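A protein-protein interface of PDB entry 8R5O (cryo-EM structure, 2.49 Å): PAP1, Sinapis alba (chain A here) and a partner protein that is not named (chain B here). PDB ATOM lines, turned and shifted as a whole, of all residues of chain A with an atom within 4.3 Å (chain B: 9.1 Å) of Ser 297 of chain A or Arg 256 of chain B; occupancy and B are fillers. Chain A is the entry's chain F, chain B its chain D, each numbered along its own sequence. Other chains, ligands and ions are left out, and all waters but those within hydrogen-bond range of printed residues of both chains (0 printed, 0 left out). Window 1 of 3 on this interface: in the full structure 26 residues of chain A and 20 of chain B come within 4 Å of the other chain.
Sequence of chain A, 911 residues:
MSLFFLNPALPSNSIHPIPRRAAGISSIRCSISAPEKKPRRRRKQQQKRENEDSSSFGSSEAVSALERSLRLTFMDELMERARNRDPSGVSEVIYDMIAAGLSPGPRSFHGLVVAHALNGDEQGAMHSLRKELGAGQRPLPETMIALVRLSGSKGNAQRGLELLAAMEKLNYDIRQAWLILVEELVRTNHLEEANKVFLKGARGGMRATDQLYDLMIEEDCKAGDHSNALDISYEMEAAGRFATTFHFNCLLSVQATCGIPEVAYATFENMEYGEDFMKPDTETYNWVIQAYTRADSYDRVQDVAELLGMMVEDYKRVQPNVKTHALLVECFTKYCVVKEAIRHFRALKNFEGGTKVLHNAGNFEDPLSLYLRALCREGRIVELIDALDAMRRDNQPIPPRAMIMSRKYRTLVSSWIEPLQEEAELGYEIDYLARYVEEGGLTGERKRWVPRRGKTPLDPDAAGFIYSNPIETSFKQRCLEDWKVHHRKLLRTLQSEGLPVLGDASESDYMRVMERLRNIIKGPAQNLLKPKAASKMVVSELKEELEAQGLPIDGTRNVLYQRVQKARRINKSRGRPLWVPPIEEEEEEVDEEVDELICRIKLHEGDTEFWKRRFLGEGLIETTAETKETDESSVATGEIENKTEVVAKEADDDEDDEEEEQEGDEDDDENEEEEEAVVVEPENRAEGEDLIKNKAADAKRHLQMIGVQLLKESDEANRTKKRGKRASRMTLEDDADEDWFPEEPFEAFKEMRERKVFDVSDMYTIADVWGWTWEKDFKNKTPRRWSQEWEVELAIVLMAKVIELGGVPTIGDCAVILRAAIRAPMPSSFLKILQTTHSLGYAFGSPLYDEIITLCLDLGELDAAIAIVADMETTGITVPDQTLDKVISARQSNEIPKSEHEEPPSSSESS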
ATOM      1  N   ALA A 295      35.718  10.911  -1.438  1.00  0.00           N
ATOM      2  CA  ALA A 295      35.779  10.734   0.003  1.00  0.00           C
ATOM      3  C   ALA A 295      36.247   9.327   0.354  1.00  0.00           C
ATOM      4  O   ALA A 295      35.972   8.358  -0.358  1.00  0.00           O
ATOM      5  CB  ALA A 295      34.412  11.000   0.631  1.00  0.00           C
ATOM      6  N   ASP A 296      36.963   9.224   1.473  1.00  0.00           N
ATOM      7  CA  ASP A 296      37.533   7.944   1.878  1.00  0.00           C
ATOM      8  C   ASP A 296      36.478   6.996   2.437  1.00  0.00           C
ATOM      9  O   ASP A 296      36.570   5.779   2.240  1.00  0.00           O
ATOM     10  CB  ASP A 296      38.645   8.169   2.901  1.00  0.00           C
ATOM     11  CG  ASP A 296      39.704   9.131   2.404  1.00  0.00           C
ATOM     12  OD1 ASP A 296      39.514   9.706   1.312  1.00  0.00           O
ATOM     13  OD2 ASP A 296      40.724   9.312   3.101  1.00  0.00           O
ATOM     14  N   SER A 297      35.473   7.523   3.134  1.00  0.00           N
ATOM     15  CA  SER A 297      34.491   6.688   3.808  1.00  0.00           C
ATOM     16  C   SER A 297      33.117   7.340   3.746  1.00  0.00           C
ATOM     17  O   SER A 297      32.970   8.501   3.357  1.00  0.00           O
ATOM     18  CB  SER A 297      34.892   6.426   5.264  1.00  0.00           C
ATOM     19  OG  SER A 297      35.195   7.637   5.932  1.00  0.00           O
ATOM     20  N   TYR A 298      32.105   6.551   4.121  1.00  0.00           N
ATOM     21  CA  TYR A 298      30.712   6.975   4.249  1.00  0.00           C
ATOM     22  C   TYR A 298      30.069   7.277   2.901  1.00  0.00           C
ATOM     23  O   TYR A 298      30.760   7.565   1.919  1.00  0.00           O
ATOM     24  CB  TYR A 298      30.596   8.186   5.180  1.00  0.00           C
ATOM     25  CG  TYR A 298      31.137   7.917   6.562  1.00  0.00           C
ATOM     26  CD1 TYR A 298      30.425   7.146   7.468  1.00  0.00           C
ATOM     27  CD2 TYR A 298      32.364   8.426   6.960  1.00  0.00           C
ATOM     28  CE1 TYR A 298      30.917   6.889   8.728  1.00  0.00           C
ATOM     29  CE2 TYR A 298      32.865   8.174   8.218  1.00  0.00           C
ATOM     30  CZ  TYR A 298      32.137   7.405   9.099  1.00  0.00           C
ATOM     31  OH  TYR A 298      32.630   7.153  10.357  1.00  0.00           O
ATOM     32  N   ARG A 300      28.286   9.436   0.232  1.00  0.00           N
ATOM     33  CA  ARG A 300      28.297  10.858  -0.084  1.00  0.00           C
ATOM     34  C   ARG A 300      27.398  11.217  -1.258  1.00  0.00           C
ATOM     35  O   ARG A 300      27.439  12.361  -1.721  1.00  0.00           O
ATOM     36  CB  ARG A 300      29.724  11.327  -0.381  1.00  0.00           C
ATOM     37  CG  ARG A 300      30.757  10.871   0.620  1.00  0.00           C
ATOM     38  CD  ARG A 300      30.594  11.567   1.952  1.00  0.00           C
ATOM     39  NE  ARG A 300      31.679  11.223   2.859  1.00  0.00           N
ATOM     40  CZ  ARG A 300      31.893  11.805   4.031  1.00  0.00           C
ATOM     41  NH1 ARG A 300      31.105  12.768   4.476  1.00  0.00           N
ATOM     42  NH2 ARG A 300      32.927  11.415   4.769  1.00  0.00           N
ATOM     43  N   TYR A 335      28.394   5.135  -7.342  1.00  0.00           N
ATOM     44  CA  TYR A 335      27.242   4.735  -6.548  1.00  0.00           C
ATOM     45  C   TYR A 335      26.191   3.998  -7.365  1.00  0.00           C
ATOM     46  O   TYR A 335      25.109   3.716  -6.841  1.00  0.00           O
ATOM     47  CB  TYR A 335      26.620   5.961  -5.874  1.00  0.00           C
ATOM     48  CG  TYR A 335      27.477   6.533  -4.770  1.00  0.00           C
ATOM     49  CD1 TYR A 335      27.336   6.096  -3.460  1.00  0.00           C
ATOM     50  CD2 TYR A 335      28.435   7.499  -5.037  1.00  0.00           C
ATOM     51  CE1 TYR A 335      28.122   6.611  -2.449  1.00  0.00           C
ATOM     52  CE2 TYR A 335      29.224   8.018  -4.033  1.00  0.00           C
ATOM     53  CZ  TYR A 335      29.063   7.572  -2.741  1.00  0.00           C
ATOM     54  OH  TYR A 335      29.848   8.089  -1.741  1.00  0.00           O
ATOM     55  N   ILE A 466      31.384   1.798  -5.101  1.00  0.00           N
ATOM     56  CA  ILE A 466      31.184   1.982  -3.667  1.00  0.00           C
ATOM     57  C   ILE A 466      30.576   0.730  -3.044  1.00  0.00           C
ATOM     58  O   ILE A 466      31.049   0.236  -2.015  1.00  0.00           O
ATOM     59  CB  ILE A 466      30.314   3.223  -3.407  1.00  0.00           C
ATOM     60  CG1 ILE A 466      30.950   4.465  -4.035  1.00  0.00           C
ATOM     61  CG2 ILE A 466      30.097   3.423  -1.923  1.00  0.00           C
ATOM     62  CD1 ILE A 466      32.335   4.765  -3.530  1.00  0.00           C
ATOM     63  N   TYR A 467      29.528   0.191  -3.666  1.00  0.00           N
ATOM     64  CA  TYR A 467      28.839  -0.984  -3.147  1.00  0.00           C
ATOM     65  C   TYR A 467      28.800  -2.089  -4.191  1.00  0.00           C
ATOM     66  O   TYR A 467      27.729  -2.636  -4.477  1.00  0.00           O
ATOM     67  CB  TYR A 467      27.410  -0.643  -2.717  1.00  0.00           C
ATOM     68  CG  TYR A 467      27.294   0.467  -1.702  1.00  0.00           C
ATOM     69  CD1 TYR A 467      27.676   0.271  -0.384  1.00  0.00           C
ATOM     70  CD2 TYR A 467      26.778   1.703  -2.057  1.00  0.00           C
ATOM     71  CE1 TYR A 467      27.562   1.281   0.546  1.00  0.00           C
ATOM     72  CE2 TYR A 467      26.661   2.719  -1.134  1.00  0.00           C
ATOM     73  CZ  TYR A 467      27.055   2.502   0.167  1.00  0.00           C
ATOM     74  OH  TYR A 467      26.938   3.513   1.092  1.00  0.00           O
ATOM     75  N   GLN B   9      35.673  16.295  15.484  1.00  0.00           N
ATOM     76  CA  GLN B   9      34.677  15.247  15.354  1.00  0.00           C
ATOM     77  C   GLN B   9      34.888  14.204  16.438  1.00  0.00           C
ATOM     78  O   GLN B   9      36.009  13.983  16.901  1.00  0.00           O
ATOM     79  CB  GLN B   9      34.743  14.574  13.978  1.00  0.00           C
ATOM     80  CG  GLN B   9      36.077  13.907  13.695  1.00  0.00           C
ATOM     81  CD  GLN B   9      36.154  13.303  12.309  1.00  0.00           C
ATOM     82  OE1 GLN B   9      35.152  13.201  11.606  1.00  0.00           O
ATOM     83  NE2 GLN B   9      37.354  12.901  11.907  1.00  0.00           N
ATOM     84  N   ARG B  11      33.336  10.069  17.158  1.00  0.00           N
ATOM     85  CA  ARG B  11      32.549   8.964  16.641  1.00  0.00           C
ATOM     86  C   ARG B  11      32.510   7.836  17.657  1.00  0.00           C
ATOM     87  O   ARG B  11      33.463   7.623  18.409  1.00  0.00           O
ATOM     88  CB  ARG B  11      33.112   8.443  15.314  1.00  0.00           C
ATOM     89  CG  ARG B  11      34.588   8.117  15.360  1.00  0.00           C
ATOM     90  CD  ARG B  11      34.980   7.181  14.236  1.00  0.00           C
ATOM     91  NE  ARG B  11      34.388   5.858  14.400  1.00  0.00           N
ATOM     92  CZ  ARG B  11      34.723   4.796  13.683  1.00  0.00           C
ATOM     93  NH1 ARG B  11      35.647   4.863  12.739  1.00  0.00           N
ATOM     94  NH2 ARG B  11      34.121   3.635  13.922  1.00  0.00           N
ATOM     95  N   LEU B 208      27.768  -9.314   2.538  1.00  0.00           N
ATOM     96  CA  LEU B 208      26.930  -8.125   2.664  1.00  0.00           C
ATOM     97  C   LEU B 208      26.457  -7.616   1.312  1.00  0.00           C
ATOM     98  O   LEU B 208      25.388  -7.002   1.221  1.00  0.00           O
ATOM     99  CB  LEU B 208      27.692  -7.029   3.404  1.00  0.00           C
ATOM    100  CG  LEU B 208      28.062  -7.349   4.851  1.00  0.00           C
ATOM    101  CD1 LEU B 208      29.072  -6.349   5.374  1.00  0.00           C
ATOM    102  CD2 LEU B 208      26.818  -7.363   5.719  1.00  0.00           C
ATOM    103  N   ARG B 209      27.232  -7.853   0.255  1.00  0.00           N
ATOM    104  CA  ARG B 209      26.811  -7.440  -1.077  1.00  0.00           C
ATOM    105  C   ARG B 209      25.715  -8.338  -1.631  1.00  0.00           C
ATOM    106  O   ARG B 209      24.878  -7.875  -2.412  1.00  0.00           O
ATOM    107  CB  ARG B 209      28.015  -7.413  -2.016  1.00  0.00           C
ATOM    108  CG  ARG B 209      29.026  -6.347  -1.644  1.00  0.00           C
ATOM    109  CD  ARG B 209      30.345  -6.536  -2.359  1.00  0.00           C
ATOM    110  NE  ARG B 209      31.253  -5.428  -2.093  1.00  0.00           N
ATOM    111  CZ  ARG B 209      32.105  -5.383  -1.080  1.00  0.00           C
ATOM    112  NH1 ARG B 209      32.205  -6.379  -0.216  1.00  0.00           N
ATOM    113  NH2 ARG B 209      32.877  -4.311  -0.929  1.00  0.00           N
ATOM    114  N   ILE B 212      22.312  -7.074  -0.170  1.00  0.00           N
ATOM    115  CA  ILE B 212      21.734  -5.904  -0.825  1.00  0.00           C
ATOM    116  C   ILE B 212      20.987  -6.305  -2.091  1.00  0.00           C
ATOM    117  O   ILE B 212      19.880  -5.819  -2.352  1.00  0.00           O
ATOM    118  CB  ILE B 212      22.831  -4.866  -1.118  1.00  0.00           C
ATOM    119  CG1 ILE B 212      23.548  -4.472   0.172  1.00  0.00           C
ATOM    120  CG2 ILE B 212      22.238  -3.641  -1.792  1.00  0.00           C
ATOM    121  CD1 ILE B 212      24.707  -3.532  -0.041  1.00  0.00           C
ATOM    122  N   GLU B 249      19.755  -1.213   4.125  1.00  0.00           N
ATOM    123  CA  GLU B 249      20.385  -0.056   4.750  1.00  0.00           C
ATOM    124  C   GLU B 249      21.458  -0.489   5.740  1.00  0.00           C
ATOM    125  O   GLU B 249      22.542   0.101   5.791  1.00  0.00           O
ATOM    126  CB  GLU B 249      19.328   0.803   5.440  1.00  0.00           C
ATOM    127  CG  GLU B 249      19.886   1.984   6.213  1.00  0.00           C
ATOM    128  CD  GLU B 249      18.812   2.748   6.964  1.00  0.00           C
ATOM    129  OE1 GLU B 249      17.621   2.398   6.823  1.00  0.00           O
ATOM    130  OE2 GLU B 249      19.159   3.699   7.696  1.00  0.00           O
ATOM    131  N   LEU B 250      21.172  -1.522   6.535  1.00  0.00           N
ATOM    132  CA  LEU B 250      22.143  -2.011   7.508  1.00  0.00           C
ATOM    133  C   LEU B 250      23.380  -2.575   6.821  1.00  0.00           C
ATOM    134  O   LEU B 250      24.509  -2.336   7.263  1.00  0.00           O
ATOM    135  CB  LEU B 250      21.493  -3.069   8.399  1.00  0.00           C
ATOM    136  CG  LEU B 250      22.168  -3.385   9.733  1.00  0.00           C
ATOM    137  CD1 LEU B 250      22.267  -2.135  10.586  1.00  0.00           C
ATOM    138  CD2 LEU B 250      21.401  -4.471  10.463  1.00  0.00           C
ATOM    139  N   ALA B 251      23.186  -3.329   5.736  1.00  0.00           N
ATOM    140  CA  ALA B 251      24.318  -3.917   5.027  1.00  0.00           C
ATOM    141  C   ALA B 251      25.222  -2.845   4.432  1.00  0.00           C
ATOM    142  O   ALA B 251      26.450  -2.982   4.447  1.00  0.00           O
ATOM    143  CB  ALA B 251      23.818  -4.860   3.933  1.00  0.00           C
ATOM    144  N   LYS B 252      24.632  -1.773   3.898  1.00  0.00           N
ATOM    145  CA  LYS B 252      25.427  -0.723   3.268  1.00  0.00           C
ATOM    146  C   LYS B 252      26.353  -0.042   4.265  1.00  0.00           C
ATOM    147  O   LYS B 252      27.505   0.264   3.941  1.00  0.00           O
ATOM    148  CB  LYS B 252      24.514   0.306   2.606  1.00  0.00           C
ATOM    149  CG  LYS B 252      23.940  -0.132   1.278  1.00  0.00           C
ATOM    150  CD  LYS B 252      23.166   0.995   0.628  1.00  0.00           C
ATOM    151  CE  LYS B 252      22.633   0.587  -0.731  1.00  0.00           C
ATOM    152  NZ  LYS B 252      21.905   1.705  -1.392  1.00  0.00           N
ATOM    153  N   HIS B 253      25.865   0.212   5.481  1.00  0.00           N
ATOM    154  CA  HIS B 253      26.683   0.903   6.473  1.00  0.00           C
ATOM    155  C   HIS B 253      27.897   0.074   6.873  1.00  0.00           C
ATOM    156  O   HIS B 253      28.981   0.623   7.099  1.00  0.00           O
ATOM    157  CB  HIS B 253      25.841   1.260   7.695  1.00  0.00           C
ATOM    158  CG  HIS B 253      24.901   2.402   7.463  1.00  0.00           C
ATOM    159  ND1 HIS B 253      23.601   2.223   7.044  1.00  0.00           N
ATOM    160  CD2 HIS B 253      25.080   3.739   7.575  1.00  0.00           C
ATOM    161  CE1 HIS B 253      23.016   3.401   6.918  1.00  0.00           C
ATOM    162  NE2 HIS B 253      23.892   4.337   7.234  1.00  0.00           N
ATOM    163  N   PHE B 254      27.741  -1.249   6.971  1.00  0.00           N
ATOM    164  CA  PHE B 254      28.882  -2.100   7.286  1.00  0.00           C
ATOM    165  C   PHE B 254      29.933  -2.047   6.184  1.00  0.00           C
ATOM    166  O   PHE B 254      31.136  -2.081   6.460  1.00  0.00           O
ATOM    167  CB  PHE B 254      28.424  -3.540   7.518  1.00  0.00           C
ATOM    168  CG  PHE B 254      27.751  -3.761   8.842  1.00  0.00           C
ATOM    169  CD1 PHE B 254      28.430  -3.530  10.025  1.00  0.00           C
ATOM    170  CD2 PHE B 254      26.449  -4.224   8.903  1.00  0.00           C
ATOM    171  CE1 PHE B 254      27.817  -3.738  11.241  1.00  0.00           C
ATOM    172  CE2 PHE B 254      25.831  -4.434  10.116  1.00  0.00           C
ATOM    173  CZ  PHE B 254      26.517  -4.192  11.287  1.00  0.00           C
ATOM    174  N   ILE B 255      29.494  -1.970   4.926  1.00  0.00           N
ATOM    175  CA  ILE B 255      30.425  -1.982   3.802  1.00  0.00           C
ATOM    176  C   ILE B 255      31.311  -0.741   3.810  1.00  0.00           C
ATOM    177  O   ILE B 255      32.526  -0.830   3.603  1.00  0.00           O
ATOM    178  CB  ILE B 255      29.651  -2.122   2.479  1.00  0.00           C
ATOM    179  CG1 ILE B 255      29.019  -3.511   2.379  1.00  0.00           C
ATOM    180  CG2 ILE B 255      30.558  -1.863   1.287  1.00  0.00           C
ATOM    181  CD1 ILE B 255      28.236  -3.729   1.110  1.00  0.00           C
ATOM    182  N   ARG B 256      30.728   0.431   4.057  1.00  0.00           N
ATOM    183  CA  ARG B 256      31.461   1.688   3.964  1.00  0.00           C
ATOM    184  C   ARG B 256      32.111   2.111   5.274  1.00  0.00           C
ATOM    185  O   ARG B 256      32.712   3.188   5.325  1.00  0.00           O
ATOM    186  CB  ARG B 256      30.537   2.805   3.471  1.00  0.00           C
ATOM    187  CG  ARG B 256      30.357   2.820   1.968  1.00  0.00           C
ATOM    188  CD  ARG B 256      31.657   3.165   1.260  1.00  0.00           C
ATOM    189  NE  ARG B 256      31.882   4.605   1.205  1.00  0.00           N
ATOM    190  CZ  ARG B 256      32.888   5.182   0.563  1.00  0.00           C
ATOM    191  NH1 ARG B 256      33.789   4.470  -0.091  1.00  0.00           N
ATOM    192  NH2 ARG B 256      32.988   6.507   0.575  1.00  0.00           N
ATOM    193  N   THR B 257      32.008   1.309   6.324  1.00  0.00           N
ATOM    194  CA  THR B 257      32.664   1.592   7.591  1.00  0.00           C
ATOM    195  C   THR B 257      33.663   0.484   7.905  1.00  0.00           C
ATOM    196  O   THR B 257      33.832  -0.469   7.142  1.00  0.00           O
ATOM    197  CB  THR B 257      31.643   1.741   8.722  1.00  0.00           C
ATOM    198  OG1 THR B 257      30.850   0.551   8.814  1.00  0.00           O
ATOM    199  CG2 THR B 257      30.737   2.937   8.470  1.00  0.00           C
ATOM    200  N   ASN B 258      34.334   0.623   9.046  1.00  0.00           N
ATOM    201  CA  ASN B 258      35.256  -0.389   9.536  1.00  0.00           C
ATOM    202  C   ASN B 258      34.644  -1.246  10.636  1.00  0.00           C
ATOM    203  O   ASN B 258      35.368  -1.981  11.314  1.00  0.00           O
ATOM    204  CB  ASN B 258      36.548   0.267  10.032  1.00  0.00           C
ATOM    205  CG  ASN B 258      36.291   1.405  10.996  1.00  0.00           C
ATOM    206  OD1 ASN B 258      35.935   1.185  12.154  1.00  0.00           O
ATOM    207  ND2 ASN B 258      36.481   2.632  10.527  1.00  0.00           N
ATOM    208  N   ILE B 259      33.331  -1.166  10.824  1.00  0.00           N
ATOM    209  CA  ILE B 259      32.643  -1.980  11.817  1.00  0.00           C
ATOM    210  C   ILE B 259      32.347  -3.347  11.215  1.00  0.00           C
ATOM    211  O   ILE B 259      31.747  -3.448  10.139  1.00  0.00           O
ATOM    212  CB  ILE B 259      31.353  -1.291  12.286  1.00  0.00           C
ATOM    213  CG1 ILE B 259      31.642   0.131  12.775  1.00  0.00           C
ATOM    214  CG2 ILE B 259      30.675  -2.111  13.368  1.00  0.00           C
ATOM    215  CD1 ILE B 259      32.574   0.198  13.956  1.00  0.00           C
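NH2 of Arg 256 of chain B sits close to O of Ser 297 of chain A (3.4 Å).
NH2 of Arg 256 of chain B sits at hydrogen-bond distance from O of Tyr 298 of chain A (2.8 Å).
Of the 16 printed residues of chain B, 4 touch a printed residue of chain A.
Hydrophobic or aromatic side chains of chain B within 4 Å of the printed part of chain A: Ile 255.
Of the 8 printed residues of chain A, 6 touch a printed residue of chain B.
Hydrophobic or aromatic side chains of chain A within 4 Å of the printed part of chain B: Tyr 298, Ile 466 and Tyr 467.
Among the printed residues, 10 pairs touch across the chains.
Among the printed residues, no Asp or Glu carboxylate lies within 4 Å of a Lys or Arg side-chain nitrogen of the other chain.
The backbone carbonyl oxygen (O) of His 253 of chain B lies within hydrogen-bond range of the side-chain hydroxyl (OG1) of Thr 257 of chain B (2.5 Å).
The backbone carbonyl oxygen (O) of Ser 297 of chain A sits at hydrogen-bond distance from the guanidinium group (NE) of Arg 300 of chain A, at 3.1 Å.
Among the printed residues, merely in contact across the chains: Tyr 467 of chain A with Arg 256 of chain B (3.5 Å), Tyr 467 of chain A with Lys 252 of chain B (3.5 Å), Ile 466 of chain A with Arg 256 of chain B (3.6 Å), Ala 295 of chain A with Arg 256 of chain B (3.6 Å), Asp 296 of chain A with Arg 256 of chain B (3.9 Å), Ile 466 of chain A with Ile 255 of chain B (3.9 Å), Tyr 467 of chain A with Ile 255 of chain B (3.96 Å) and Tyr 298 of chain A with Thr 257 of chain B (3.96 Å).
Printed residues of chain B within 4 Å of Ser 297 of chain A: Arg 256.
Of chain A, only Ala 295 (3.6 Å), Asp 296 (3.9 Å), Ser 297 (3.3 Å), Tyr 298 (2.8 Å), Ile 466 (3.6 Å) and Tyr 467 (3.5 Å) come within 4 Å of Arg 256 of chain B.
Printed residues of chain B within 4 Å of Tyr 467 of chain A: Lys 252, Ile 255 and Arg 256.
Of the printed residues of chain B, Ile 466 of chain A touches Ile 255 (3.9 Å) and Arg 256 (3.6 Å).
Of the printed residues of chain A, Thr 257 of chain B touches Tyr 298.
Printed residues of chain B within 4 Å of Ala 295 of chain A: Arg 256 (3.6 Å).
Of the printed residues of chain B, Tyr 298 of chain A touches Arg 256 and Thr 257.
Tyr 335 of chain A touches none of the printed residues of chain B.
The nearest residue of chain B that does not touch Ser 297 of chain A is Thr 257 of chain B (5.8 Å).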
